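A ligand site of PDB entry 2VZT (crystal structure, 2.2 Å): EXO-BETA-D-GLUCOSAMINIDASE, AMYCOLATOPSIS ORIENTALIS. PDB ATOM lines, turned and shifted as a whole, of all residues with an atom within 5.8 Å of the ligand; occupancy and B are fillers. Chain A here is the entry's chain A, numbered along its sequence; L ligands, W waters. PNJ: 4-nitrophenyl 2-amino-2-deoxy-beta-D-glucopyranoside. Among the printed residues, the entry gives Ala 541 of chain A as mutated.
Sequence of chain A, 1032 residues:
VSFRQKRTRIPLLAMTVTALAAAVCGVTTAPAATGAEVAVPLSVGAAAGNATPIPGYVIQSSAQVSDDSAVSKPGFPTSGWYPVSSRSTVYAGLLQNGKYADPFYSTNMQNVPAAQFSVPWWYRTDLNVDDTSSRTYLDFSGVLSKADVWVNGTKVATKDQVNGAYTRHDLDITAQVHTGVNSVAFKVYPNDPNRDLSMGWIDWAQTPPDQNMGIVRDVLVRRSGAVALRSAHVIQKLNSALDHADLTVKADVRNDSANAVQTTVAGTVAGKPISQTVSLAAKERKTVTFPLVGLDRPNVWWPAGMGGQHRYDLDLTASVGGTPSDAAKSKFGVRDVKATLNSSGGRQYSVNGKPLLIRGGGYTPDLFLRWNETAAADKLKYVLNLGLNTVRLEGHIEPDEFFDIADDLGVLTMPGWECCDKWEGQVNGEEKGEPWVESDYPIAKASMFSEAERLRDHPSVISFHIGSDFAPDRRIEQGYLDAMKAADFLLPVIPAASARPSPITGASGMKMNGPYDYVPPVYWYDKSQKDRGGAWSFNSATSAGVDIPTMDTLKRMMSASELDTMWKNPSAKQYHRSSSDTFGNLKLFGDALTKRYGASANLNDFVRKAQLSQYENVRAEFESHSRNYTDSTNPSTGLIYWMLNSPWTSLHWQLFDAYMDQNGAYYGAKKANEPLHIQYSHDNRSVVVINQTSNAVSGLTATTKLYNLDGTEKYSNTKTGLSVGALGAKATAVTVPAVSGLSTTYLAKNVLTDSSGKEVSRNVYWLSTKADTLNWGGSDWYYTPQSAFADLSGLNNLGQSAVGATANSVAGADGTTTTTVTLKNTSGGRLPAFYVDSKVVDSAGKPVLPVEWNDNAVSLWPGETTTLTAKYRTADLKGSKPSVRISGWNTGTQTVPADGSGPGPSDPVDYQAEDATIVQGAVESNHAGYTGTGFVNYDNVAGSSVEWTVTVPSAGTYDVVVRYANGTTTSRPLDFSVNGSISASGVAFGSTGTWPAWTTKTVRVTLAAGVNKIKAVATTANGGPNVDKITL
The side-chain carboxylate (OD2) of Asp 203 sits at hydrogen-bond distance from an oxygen (O6) of the ligand (2.5 Å). OE2 of Glu 394 is in salt-bridge range of N2 of the ligand (3.1 Å). The indole nitrogen (NE1) of Trp 642 is in hydrogen-bond range of an oxygen (O4) of the ligand (3.0 Å). NE1 of Trp 204 sits at hydrogen-bond distance from O3 of the ligand (3.0 Å). The side-chain sulfur (SD) of Met 512 sits at hydrogen-bond distance from a nitrogen (N2) of the ligand (3.7 Å). SG of Cys 419 lies within hydrogen-bond range of N2 of the ligand (3.5 Å).
Ile 202 touches the ligand (CD1 to O3, 3.6 Å). Ser 468 touches the ligand. Asp 469 touches the ligand (OD2 to C8, 3.5 Å). Asn 513 touches the ligand (C to O7, 3.8 Å). Gly 514 touches the ligand (N to O7, 3.9 Å). Tyr 516 touches the ligand (OH to C12, 3.1 Å). CE2 of Phe 583 touches O6 of the ligand, at 3.7 Å. Trp 653 touches the ligand. CH2 of Trp 781 touches O6 of the ligand, 3.3 Å away. Hydrophobic or aromatic side chains within 4 Å of the ligand: Ile 202, Trp 204, Met 512, Tyr 516, Phe 583, Trp 642, Trp 653 and Trp 781. 15 residues have an atom within 4 Å of the ligand: Ile 202, Asp 203, Trp 204, Glu 394, Cys 419, Ser 468, Asp 469, Met 512, Asn 513, Gly 514, Tyr 516, Phe 583, Trp 642, Trp 653 and Trp 781.
The backbone NH of Cys 419 sits at hydrogen-bond distance from the side-chain carboxylate of Glu 394 (3.1 Å). OE2 of Glu 394 sits at hydrogen-bond distance from OG of Ser 468. O of Tyr 516 is in hydrogen-bond range of NE1 of Trp 653, 3.1 Å away. The side-chain hydroxyl (OH) of Tyr 516 is in hydrogen-bond range of the backbone carbonyl oxygen (O) of Ala 541 (2.7 Å). N of Tyr 516 lies within hydrogen-bond range of O of Tyr 782. SG of Cys 420 is disulfide-bonded to SG of Cys 419 (2.1 Å). The backbone NH (N) of Met 643 is in hydrogen-bond range of the backbone carbonyl oxygen (O) of Trp 653. OG of Ser 468 is in hydrogen-bond range of NH2 of Arg 392.
Water W1 lies within hydrogen-bond range of NH1 of Arg 392 (2.7 Å), N2 of the ligand (2.7 Å), OE1 of Glu 394 (3.0 Å) and SD of Met 512 (3.5 Å).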
ATOM      1  N   ILE A 202     -18.144   5.027 -23.839  1.00  0.00           N
ATOM      2  CA  ILE A 202     -19.311   5.557 -23.146  1.00  0.00           C
ATOM      3  C   ILE A 202     -19.187   5.262 -21.652  1.00  0.00           C
ATOM      4  O   ILE A 202     -18.267   5.781 -20.995  1.00  0.00           O
ATOM      5  CB  ILE A 202     -20.660   5.070 -23.827  1.00  0.00           C
ATOM      6  CG1 ILE A 202     -20.578   5.351 -25.350  1.00  0.00           C
ATOM      7  CG2 ILE A 202     -21.930   5.729 -23.161  1.00  0.00           C
ATOM      8  CD1 ILE A 202     -21.549   4.568 -26.267  1.00  0.00           C
ATOM      9  N   ASP A 203     -20.044   4.406 -21.111  1.00  0.00           N
ATOM     10  CA  ASP A 203     -19.931   3.996 -19.719  1.00  0.00           C
ATOM     11  C   ASP A 203     -19.913   2.460 -19.595  1.00  0.00           C
ATOM     12  O   ASP A 203     -20.181   1.909 -18.520  1.00  0.00           O
ATOM     13  CB  ASP A 203     -21.076   4.613 -18.902  1.00  0.00           C
ATOM     14  CG  ASP A 203     -22.446   4.223 -19.415  1.00  0.00           C
ATOM     15  OD1 ASP A 203     -22.499   3.437 -20.401  1.00  0.00           O
ATOM     16  OD2 ASP A 203     -23.470   4.699 -18.847  1.00  0.00           O
ATOM     17  N   TRP A 204     -19.585   1.779 -20.689  1.00  0.00           N
ATOM     18  CA  TRP A 204     -19.653   0.327 -20.722  1.00  0.00           C
ATOM     19  C   TRP A 204     -18.600  -0.332 -19.864  1.00  0.00           C
ATOM     20  O   TRP A 204     -18.836  -1.418 -19.310  1.00  0.00           O
ATOM     21  CB  TRP A 204     -19.526  -0.194 -22.165  1.00  0.00           C
ATOM     22  CG  TRP A 204     -20.579   0.317 -23.120  1.00  0.00           C
ATOM     23  CD1 TRP A 204     -21.684   1.099 -22.821  1.00  0.00           C
ATOM     24  CD2 TRP A 204     -20.639   0.078 -24.527  1.00  0.00           C
ATOM     25  NE1 TRP A 204     -22.405   1.368 -23.975  1.00  0.00           N
ATOM     26  CE2 TRP A 204     -21.798   0.740 -25.028  1.00  0.00           C
ATOM     27  CE3 TRP A 204     -19.825  -0.640 -25.424  1.00  0.00           C
ATOM     28  CZ2 TRP A 204     -22.142   0.724 -26.386  1.00  0.00           C
ATOM     29  CZ3 TRP A 204     -20.184  -0.669 -26.772  1.00  0.00           C
ATOM     30  CH2 TRP A 204     -21.338   0.001 -27.234  1.00  0.00           C
ATOM     31  N   ARG A 392     -27.430  -5.610 -31.775  1.00  0.00           N
ATOM     32  CA  ARG A 392     -27.259  -4.202 -32.066  1.00  0.00           C
ATOM     33  C   ARG A 392     -25.794  -3.878 -31.908  1.00  0.00           C
ATOM     34  O   ARG A 392     -25.150  -4.350 -30.967  1.00  0.00           O
ATOM     35  CB  ARG A 392     -28.122  -3.341 -31.114  1.00  0.00           C
ATOM     36  CG  ARG A 392     -28.255  -1.923 -31.584  1.00  0.00           C
ATOM     37  CD  ARG A 392     -29.102  -1.060 -30.675  1.00  0.00           C
ATOM     38  NE  ARG A 392     -28.655   0.330 -30.821  1.00  0.00           N
ATOM     39  CZ  ARG A 392     -28.630   1.229 -29.825  1.00  0.00           C
ATOM     40  NH1 ARG A 392     -29.058   0.894 -28.606  1.00  0.00           N
ATOM     41  NH2 ARG A 392     -28.175   2.461 -30.077  1.00  0.00           N
ATOM     42  N   GLU A 394     -24.050  -0.509 -31.283  1.00  0.00           N
ATOM     43  CA  GLU A 394     -23.934   0.929 -31.043  1.00  0.00           C
ATOM     44  C   GLU A 394     -22.486   1.399 -31.256  1.00  0.00           C
ATOM     45  O   GLU A 394     -21.628   1.312 -30.349  1.00  0.00           O
ATOM     46  CB  GLU A 394     -24.504   1.357 -29.686  1.00  0.00           C
ATOM     47  CG  GLU A 394     -24.456   2.888 -29.533  1.00  0.00           C
ATOM     48  CD  GLU A 394     -24.856   3.406 -28.160  1.00  0.00           C
ATOM     49  OE1 GLU A 394     -24.824   2.613 -27.213  1.00  0.00           O
ATOM     50  OE2 GLU A 394     -25.171   4.613 -28.039  1.00  0.00           O
ATOM     51  N   CYS A 419     -23.720   7.100 -29.102  1.00  0.00           N
ATOM     52  CA  CYS A 419     -24.088   8.320 -28.359  1.00  0.00           C
ATOM     53  C   CYS A 419     -22.879   8.862 -27.626  1.00  0.00           C
ATOM     54  O   CYS A 419     -21.778   8.270 -27.654  1.00  0.00           O
ATOM     55  CB  CYS A 419     -25.179   8.044 -27.304  1.00  0.00           C
ATOM     56  SG  CYS A 419     -24.581   7.287 -25.727  1.00  0.00           S
ATOM     57  N   CYS A 420     -23.106  10.006 -26.971  1.00  0.00           N
ATOM     58  CA  CYS A 420     -22.301  10.400 -25.811  1.00  0.00           C
ATOM     59  C   CYS A 420     -20.838  10.724 -26.134  1.00  0.00           C
ATOM     60  O   CYS A 420     -19.983  10.677 -25.252  1.00  0.00           O
ATOM     61  CB  CYS A 420     -22.411   9.293 -24.731  1.00  0.00           C
ATOM     62  SG  CYS A 420     -24.164   8.867 -24.428  1.00  0.00           S
ATOM     63  N   SER A 468     -28.343   7.911 -31.956  1.00  0.00           N
ATOM     64  CA  SER A 468     -28.511   6.999 -30.850  1.00  0.00           C
ATOM     65  C   SER A 468     -29.547   7.221 -29.723  1.00  0.00           C
ATOM     66  O   SER A 468     -30.692   6.812 -29.873  1.00  0.00           O
ATOM     67  CB  SER A 468     -27.158   6.465 -30.327  1.00  0.00           C
ATOM     68  OG  SER A 468     -27.328   5.462 -29.337  1.00  0.00           O
ATOM     69  N   ASP A 469     -29.243   7.834 -28.596  1.00  0.00           N
ATOM     70  CA  ASP A 469     -29.583   9.184 -28.115  1.00  0.00           C
ATOM     71  C   ASP A 469     -30.197  10.346 -28.921  1.00  0.00           C
ATOM     72  O   ASP A 469     -31.401  10.305 -29.237  1.00  0.00           O
ATOM     73  CB  ASP A 469     -28.751   9.599 -26.889  1.00  0.00           C
ATOM     74  CG  ASP A 469     -29.605  10.272 -25.800  1.00  0.00           C
ATOM     75  OD1 ASP A 469     -30.858  10.168 -25.865  1.00  0.00           O
ATOM     76  OD2 ASP A 469     -29.028  10.909 -24.878  1.00  0.00           O
ATOM     77  N   ARG A 500     -36.439  10.223 -29.552  1.00  0.00           N
ATOM     78  CA  ARG A 500     -36.205  11.499 -30.249  1.00  0.00           C
ATOM     79  C   ARG A 500     -36.298  11.416 -31.781  1.00  0.00           C
ATOM     80  O   ARG A 500     -35.626  10.573 -32.378  1.00  0.00           O
ATOM     81  CB  ARG A 500     -34.859  12.089 -29.840  1.00  0.00           C
ATOM     82  CG  ARG A 500     -34.705  12.302 -28.332  1.00  0.00           C
ATOM     83  CD  ARG A 500     -33.318  12.839 -27.996  1.00  0.00           C
ATOM     84  NE  ARG A 500     -33.377  13.806 -26.896  1.00  0.00           N
ATOM     85  CZ  ARG A 500     -33.065  13.522 -25.645  1.00  0.00           C
ATOM     86  NH1 ARG A 500     -32.642  12.283 -25.340  1.00  0.00           N
ATOM     87  NH2 ARG A 500     -33.163  14.456 -24.705  1.00  0.00           N
ATOM     88  N   MET A 512     -35.532   4.720 -25.166  1.00  0.00           N
ATOM     89  CA  MET A 512     -34.507   4.445 -24.157  1.00  0.00           C
ATOM     90  C   MET A 512     -34.889   5.175 -22.866  1.00  0.00           C
ATOM     91  O   MET A 512     -34.369   6.238 -22.574  1.00  0.00           O
ATOM     92  CB  MET A 512     -33.101   4.880 -24.627  1.00  0.00           C
ATOM     93  CG  MET A 512     -32.432   3.886 -25.586  1.00  0.00           C
ATOM     94  SD  MET A 512     -30.703   4.136 -25.959  1.00  0.00           S
ATOM     95  CE  MET A 512     -30.656   5.823 -26.558  1.00  0.00           C
ATOM     96  N   ASN A 513     -35.820   4.585 -22.118  1.00  0.00           N
ATOM     97  CA  ASN A 513     -36.372   5.189 -20.898  1.00  0.00           C
ATOM     98  C   ASN A 513     -35.741   4.602 -19.645  1.00  0.00           C
ATOM     99  O   ASN A 513     -36.261   4.813 -18.512  1.00  0.00           O
ATOM    100  CB  ASN A 513     -37.872   4.907 -20.810  1.00  0.00           C
ATOM    101  CG  ASN A 513     -38.701   5.751 -21.769  1.00  0.00           C
ATOM    102  OD1 ASN A 513     -38.268   6.772 -22.249  1.00  0.00           O
ATOM    103  ND2 ASN A 513     -39.908   5.307 -22.029  1.00  0.00           N
ATOM    104  N   GLY A 514     -34.637   3.863 -19.843  1.00  0.00           N
ATOM    105  CA  GLY A 514     -34.141   2.957 -18.819  1.00  0.00           C
ATOM    106  C   GLY A 514     -35.058   1.729 -18.698  1.00  0.00           C
ATOM    107  O   GLY A 514     -36.046   1.594 -19.436  1.00  0.00           O
ATOM    108  N   TYR A 516     -31.297   0.556 -16.413  1.00  0.00           N
ATOM    109  CA  TYR A 516     -29.930   0.043 -16.579  1.00  0.00           C
ATOM    110  C   TYR A 516     -29.413  -0.509 -15.248  1.00  0.00           C
ATOM    111  O   TYR A 516     -28.237  -0.856 -15.131  1.00  0.00           O
ATOM    112  CB  TYR A 516     -28.993   1.143 -17.077  1.00  0.00           C
ATOM    113  CG  TYR A 516     -29.365   1.598 -18.465  1.00  0.00           C
ATOM    114  CD1 TYR A 516     -28.948   0.853 -19.610  1.00  0.00           C
ATOM    115  CD2 TYR A 516     -30.199   2.721 -18.653  1.00  0.00           C
ATOM    116  CE1 TYR A 516     -29.300   1.254 -20.894  1.00  0.00           C
ATOM    117  CE2 TYR A 516     -30.571   3.126 -19.945  1.00  0.00           C
ATOM    118  CZ  TYR A 516     -30.120   2.363 -21.071  1.00  0.00           C
ATOM    119  OH  TYR A 516     -30.473   2.745 -22.361  1.00  0.00           O
ATOM    120  N   ALA A 541     -32.276  -0.704 -25.743  1.00  0.00           N
ATOM    121  CA  ALA A 541     -31.088  -0.760 -24.865  1.00  0.00           C
ATOM    122  C   ALA A 541     -31.514  -0.738 -23.405  1.00  0.00           C
ATOM    123  O   ALA A 541     -31.617   0.338 -22.793  1.00  0.00           O
ATOM    124  CB  ALA A 541     -30.097   0.418 -25.145  1.00  0.00           C
ATOM    125  N   PHE A 583     -22.868   4.161 -12.381  1.00  0.00           N
ATOM    126  CA  PHE A 583     -22.753   2.697 -12.407  1.00  0.00           C
ATOM    127  C   PHE A 583     -21.419   2.220 -11.861  1.00  0.00           C
ATOM    128  O   PHE A 583     -20.884   1.225 -12.312  1.00  0.00           O
ATOM    129  CB  PHE A 583     -22.999   2.142 -13.839  1.00  0.00           C
ATOM    130  CG  PHE A 583     -24.275   2.674 -14.476  1.00  0.00           C
ATOM    131  CD1 PHE A 583     -25.535   2.309 -13.990  1.00  0.00           C
ATOM    132  CD2 PHE A 583     -24.219   3.536 -15.567  1.00  0.00           C
ATOM    133  CE1 PHE A 583     -26.698   2.782 -14.557  1.00  0.00           C
ATOM    134  CE2 PHE A 583     -25.381   4.019 -16.130  1.00  0.00           C
ATOM    135  CZ  PHE A 583     -26.643   3.627 -15.623  1.00  0.00           C
ATOM    136  N   TRP A 642     -29.224  -5.020 -22.619  1.00  0.00           N
ATOM    137  CA  TRP A 642     -27.988  -4.232 -22.461  1.00  0.00           C
ATOM    138  C   TRP A 642     -27.080  -4.953 -21.475  1.00  0.00           C
ATOM    139  O   TRP A 642     -27.339  -4.912 -20.251  1.00  0.00           O
ATOM    140  CB  TRP A 642     -28.323  -2.807 -21.987  1.00  0.00           C
ATOM    141  CG  TRP A 642     -27.394  -1.762 -22.540  1.00  0.00           C
ATOM    142  CD1 TRP A 642     -26.609  -0.914 -21.837  1.00  0.00           C
ATOM    143  CD2 TRP A 642     -27.102  -1.532 -23.940  1.00  0.00           C
ATOM    144  NE1 TRP A 642     -25.865  -0.132 -22.695  1.00  0.00           N
ATOM    145  CE2 TRP A 642     -26.152  -0.496 -23.991  1.00  0.00           C
ATOM    146  CE3 TRP A 642     -27.584  -2.092 -25.136  1.00  0.00           C
ATOM    147  CZ2 TRP A 642     -25.640   0.003 -25.215  1.00  0.00           C
ATOM    148  CZ3 TRP A 642     -27.076  -1.625 -26.325  1.00  0.00           C
ATOM    149  CH2 TRP A 642     -26.118  -0.562 -26.361  1.00  0.00           C
ATOM    150  N   MET A 643     -26.042  -5.673 -21.930  1.00  0.00           N
ATOM    151  CA  MET A 643     -25.693  -5.947 -23.337  1.00  0.00           C
ATOM    152  C   MET A 643     -25.518  -7.451 -23.519  1.00  0.00           C
ATOM    153  O   MET A 643     -25.505  -8.186 -22.519  1.00  0.00           O
ATOM    154  CB  MET A 643     -24.378  -5.228 -23.690  1.00  0.00           C
ATOM    155  CG  MET A 643     -24.410  -3.776 -23.293  1.00  0.00           C
ATOM    156  SD  MET A 643     -23.135  -2.731 -23.987  1.00  0.00           S
ATOM    157  CE  MET A 643     -23.307  -1.501 -22.800  1.00  0.00           C
ATOM    158  N   TRP A 653     -24.151  -5.826 -17.362  1.00  0.00           N
ATOM    159  CA  TRP A 653     -24.482  -5.597 -18.771  1.00  0.00           C
ATOM    160  C   TRP A 653     -23.807  -6.655 -19.661  1.00  0.00           C
ATOM    161  O   TRP A 653     -23.112  -6.318 -20.633  1.00  0.00           O
ATOM    162  CB  TRP A 653     -24.076  -4.162 -19.232  1.00  0.00           C
ATOM    163  CG  TRP A 653     -24.719  -2.995 -18.433  1.00  0.00           C
ATOM    164  CD1 TRP A 653     -25.712  -3.069 -17.511  1.00  0.00           C
ATOM    165  CD2 TRP A 653     -24.419  -1.584 -18.589  1.00  0.00           C
ATOM    166  NE1 TRP A 653     -26.029  -1.801 -17.038  1.00  0.00           N
ATOM    167  CE2 TRP A 653     -25.269  -0.880 -17.706  1.00  0.00           C
ATOM    168  CE3 TRP A 653     -23.525  -0.868 -19.399  1.00  0.00           C
ATOM    169  CZ2 TRP A 653     -25.229   0.518 -17.594  1.00  0.00           C
ATOM    170  CZ3 TRP A 653     -23.492   0.523 -19.297  1.00  0.00           C
ATOM    171  CH2 TRP A 653     -24.338   1.201 -18.398  1.00  0.00           C
ATOM    172  N   TRP A 781     -33.764   8.109 -14.319  1.00  0.00           N
ATOM    173  CA  TRP A 781     -33.660   7.700 -15.715  1.00  0.00           C
ATOM    174  C   TRP A 781     -33.243   6.227 -15.843  1.00  0.00           C
ATOM    175  O   TRP A 781     -33.668   5.536 -16.758  1.00  0.00           O
ATOM    176  CB  TRP A 781     -32.716   8.628 -16.509  1.00  0.00           C
ATOM    177  CG  TRP A 781     -31.233   8.534 -16.150  1.00  0.00           C
ATOM    178  CD1 TRP A 781     -30.584   9.221 -15.164  1.00  0.00           C
ATOM    179  CD2 TRP A 781     -30.236   7.738 -16.793  1.00  0.00           C
ATOM    180  NE1 TRP A 781     -29.246   8.895 -15.149  1.00  0.00           N
ATOM    181  CE2 TRP A 781     -29.010   7.979 -16.142  1.00  0.00           C
ATOM    182  CE3 TRP A 781     -30.258   6.834 -17.880  1.00  0.00           C
ATOM    183  CZ2 TRP A 781     -27.813   7.345 -16.532  1.00  0.00           C
ATOM    184  CZ3 TRP A 781     -29.089   6.207 -18.254  1.00  0.00           C
ATOM    185  CH2 TRP A 781     -27.883   6.477 -17.588  1.00  0.00           C
ATOM    186  N   TYR A 782     -32.406   5.752 -14.928  1.00  0.00           N
ATOM    187  CA  TYR A 782     -31.764   4.445 -15.096  1.00  0.00           C
ATOM    188  C   TYR A 782     -32.382   3.340 -14.231  1.00  0.00           C
ATOM    189  O   TYR A 782     -31.937   2.211 -14.291  1.00  0.00           O
ATOM    190  CB  TYR A 782     -30.262   4.548 -14.839  1.00  0.00           C
ATOM    191  CG  TYR A 782     -29.930   4.926 -13.425  1.00  0.00           C
ATOM    192  CD1 TYR A 782     -29.694   3.932 -12.444  1.00  0.00           C
ATOM    193  CD2 TYR A 782     -29.855   6.269 -13.039  1.00  0.00           C
ATOM    194  CE1 TYR A 782     -29.402   4.289 -11.128  1.00  0.00           C
ATOM    195  CE2 TYR A 782     -29.577   6.622 -11.740  1.00  0.00           C
ATOM    196  CZ  TYR A 782     -29.346   5.639 -10.793  1.00  0.00           C
ATOM    197  OH  TYR A 782     -29.070   6.031  -9.519  1.00  0.00           O
HETATM  198  C1  PNJ L   1     -27.800   4.938 -23.319  1.00  0.00           C
HETATM  199  C2  PNJ L   1     -26.590   4.776 -24.232  1.00  0.00           C
HETATM  200  C4  PNJ L   1     -25.421   3.625 -22.367  1.00  0.00           C
HETATM  201  C5  PNJ L   1     -26.750   3.755 -21.568  1.00  0.00           C
HETATM  202  C6  PNJ L   1     -26.614   3.733 -20.042  1.00  0.00           C
HETATM  203  C7  PNJ L   1     -29.400   6.625 -23.007  1.00  0.00           C
HETATM  204  C8  PNJ L   1     -29.767   7.943 -23.137  1.00  0.00           C
HETATM  205  C9  PNJ L   1     -30.845   8.450 -22.423  1.00  0.00           C
HETATM  206  C10 PNJ L   1     -31.549   7.633 -21.558  1.00  0.00           C
HETATM  207  C11 PNJ L   1     -31.192   6.281 -21.417  1.00  0.00           C
HETATM  208  C12 PNJ L   1     -30.112   5.797 -22.139  1.00  0.00           C
HETATM  209  N1  PNJ L   1     -32.571   8.193 -20.891  1.00  0.00           N
HETATM  210  O1  PNJ L   1     -28.302   6.201 -23.725  1.00  0.00           O
HETATM  211  O3  PNJ L   1     -24.534   3.407 -24.545  1.00  0.00           O
HETATM  212  O4  PNJ L   1     -24.639   2.496 -21.978  1.00  0.00           O
HETATM  213  C3  PNJ L   1     -25.782   3.510 -23.844  1.00  0.00           C
HETATM  214  O5  PNJ L   1     -27.366   5.002 -22.000  1.00  0.00           O
HETATM  215  O6  PNJ L   1     -25.845   4.860 -19.663  1.00  0.00           O
HETATM  216  O7  PNJ L   1     -33.367   7.498 -19.996  1.00  0.00           O
HETATM  217  N2  PNJ L   1     -27.069   4.830 -25.621  1.00  0.00           N
HETATM  218  O8  PNJ L   1     -32.834   9.521 -21.145  1.00  0.00           O
HETATM  219  O   HOH W   1     -27.767   2.464 -26.826  1.00  0.00           O
HETATM  220  O   HOH W   2     -26.138   7.710 -20.645  1.00  0.00           O
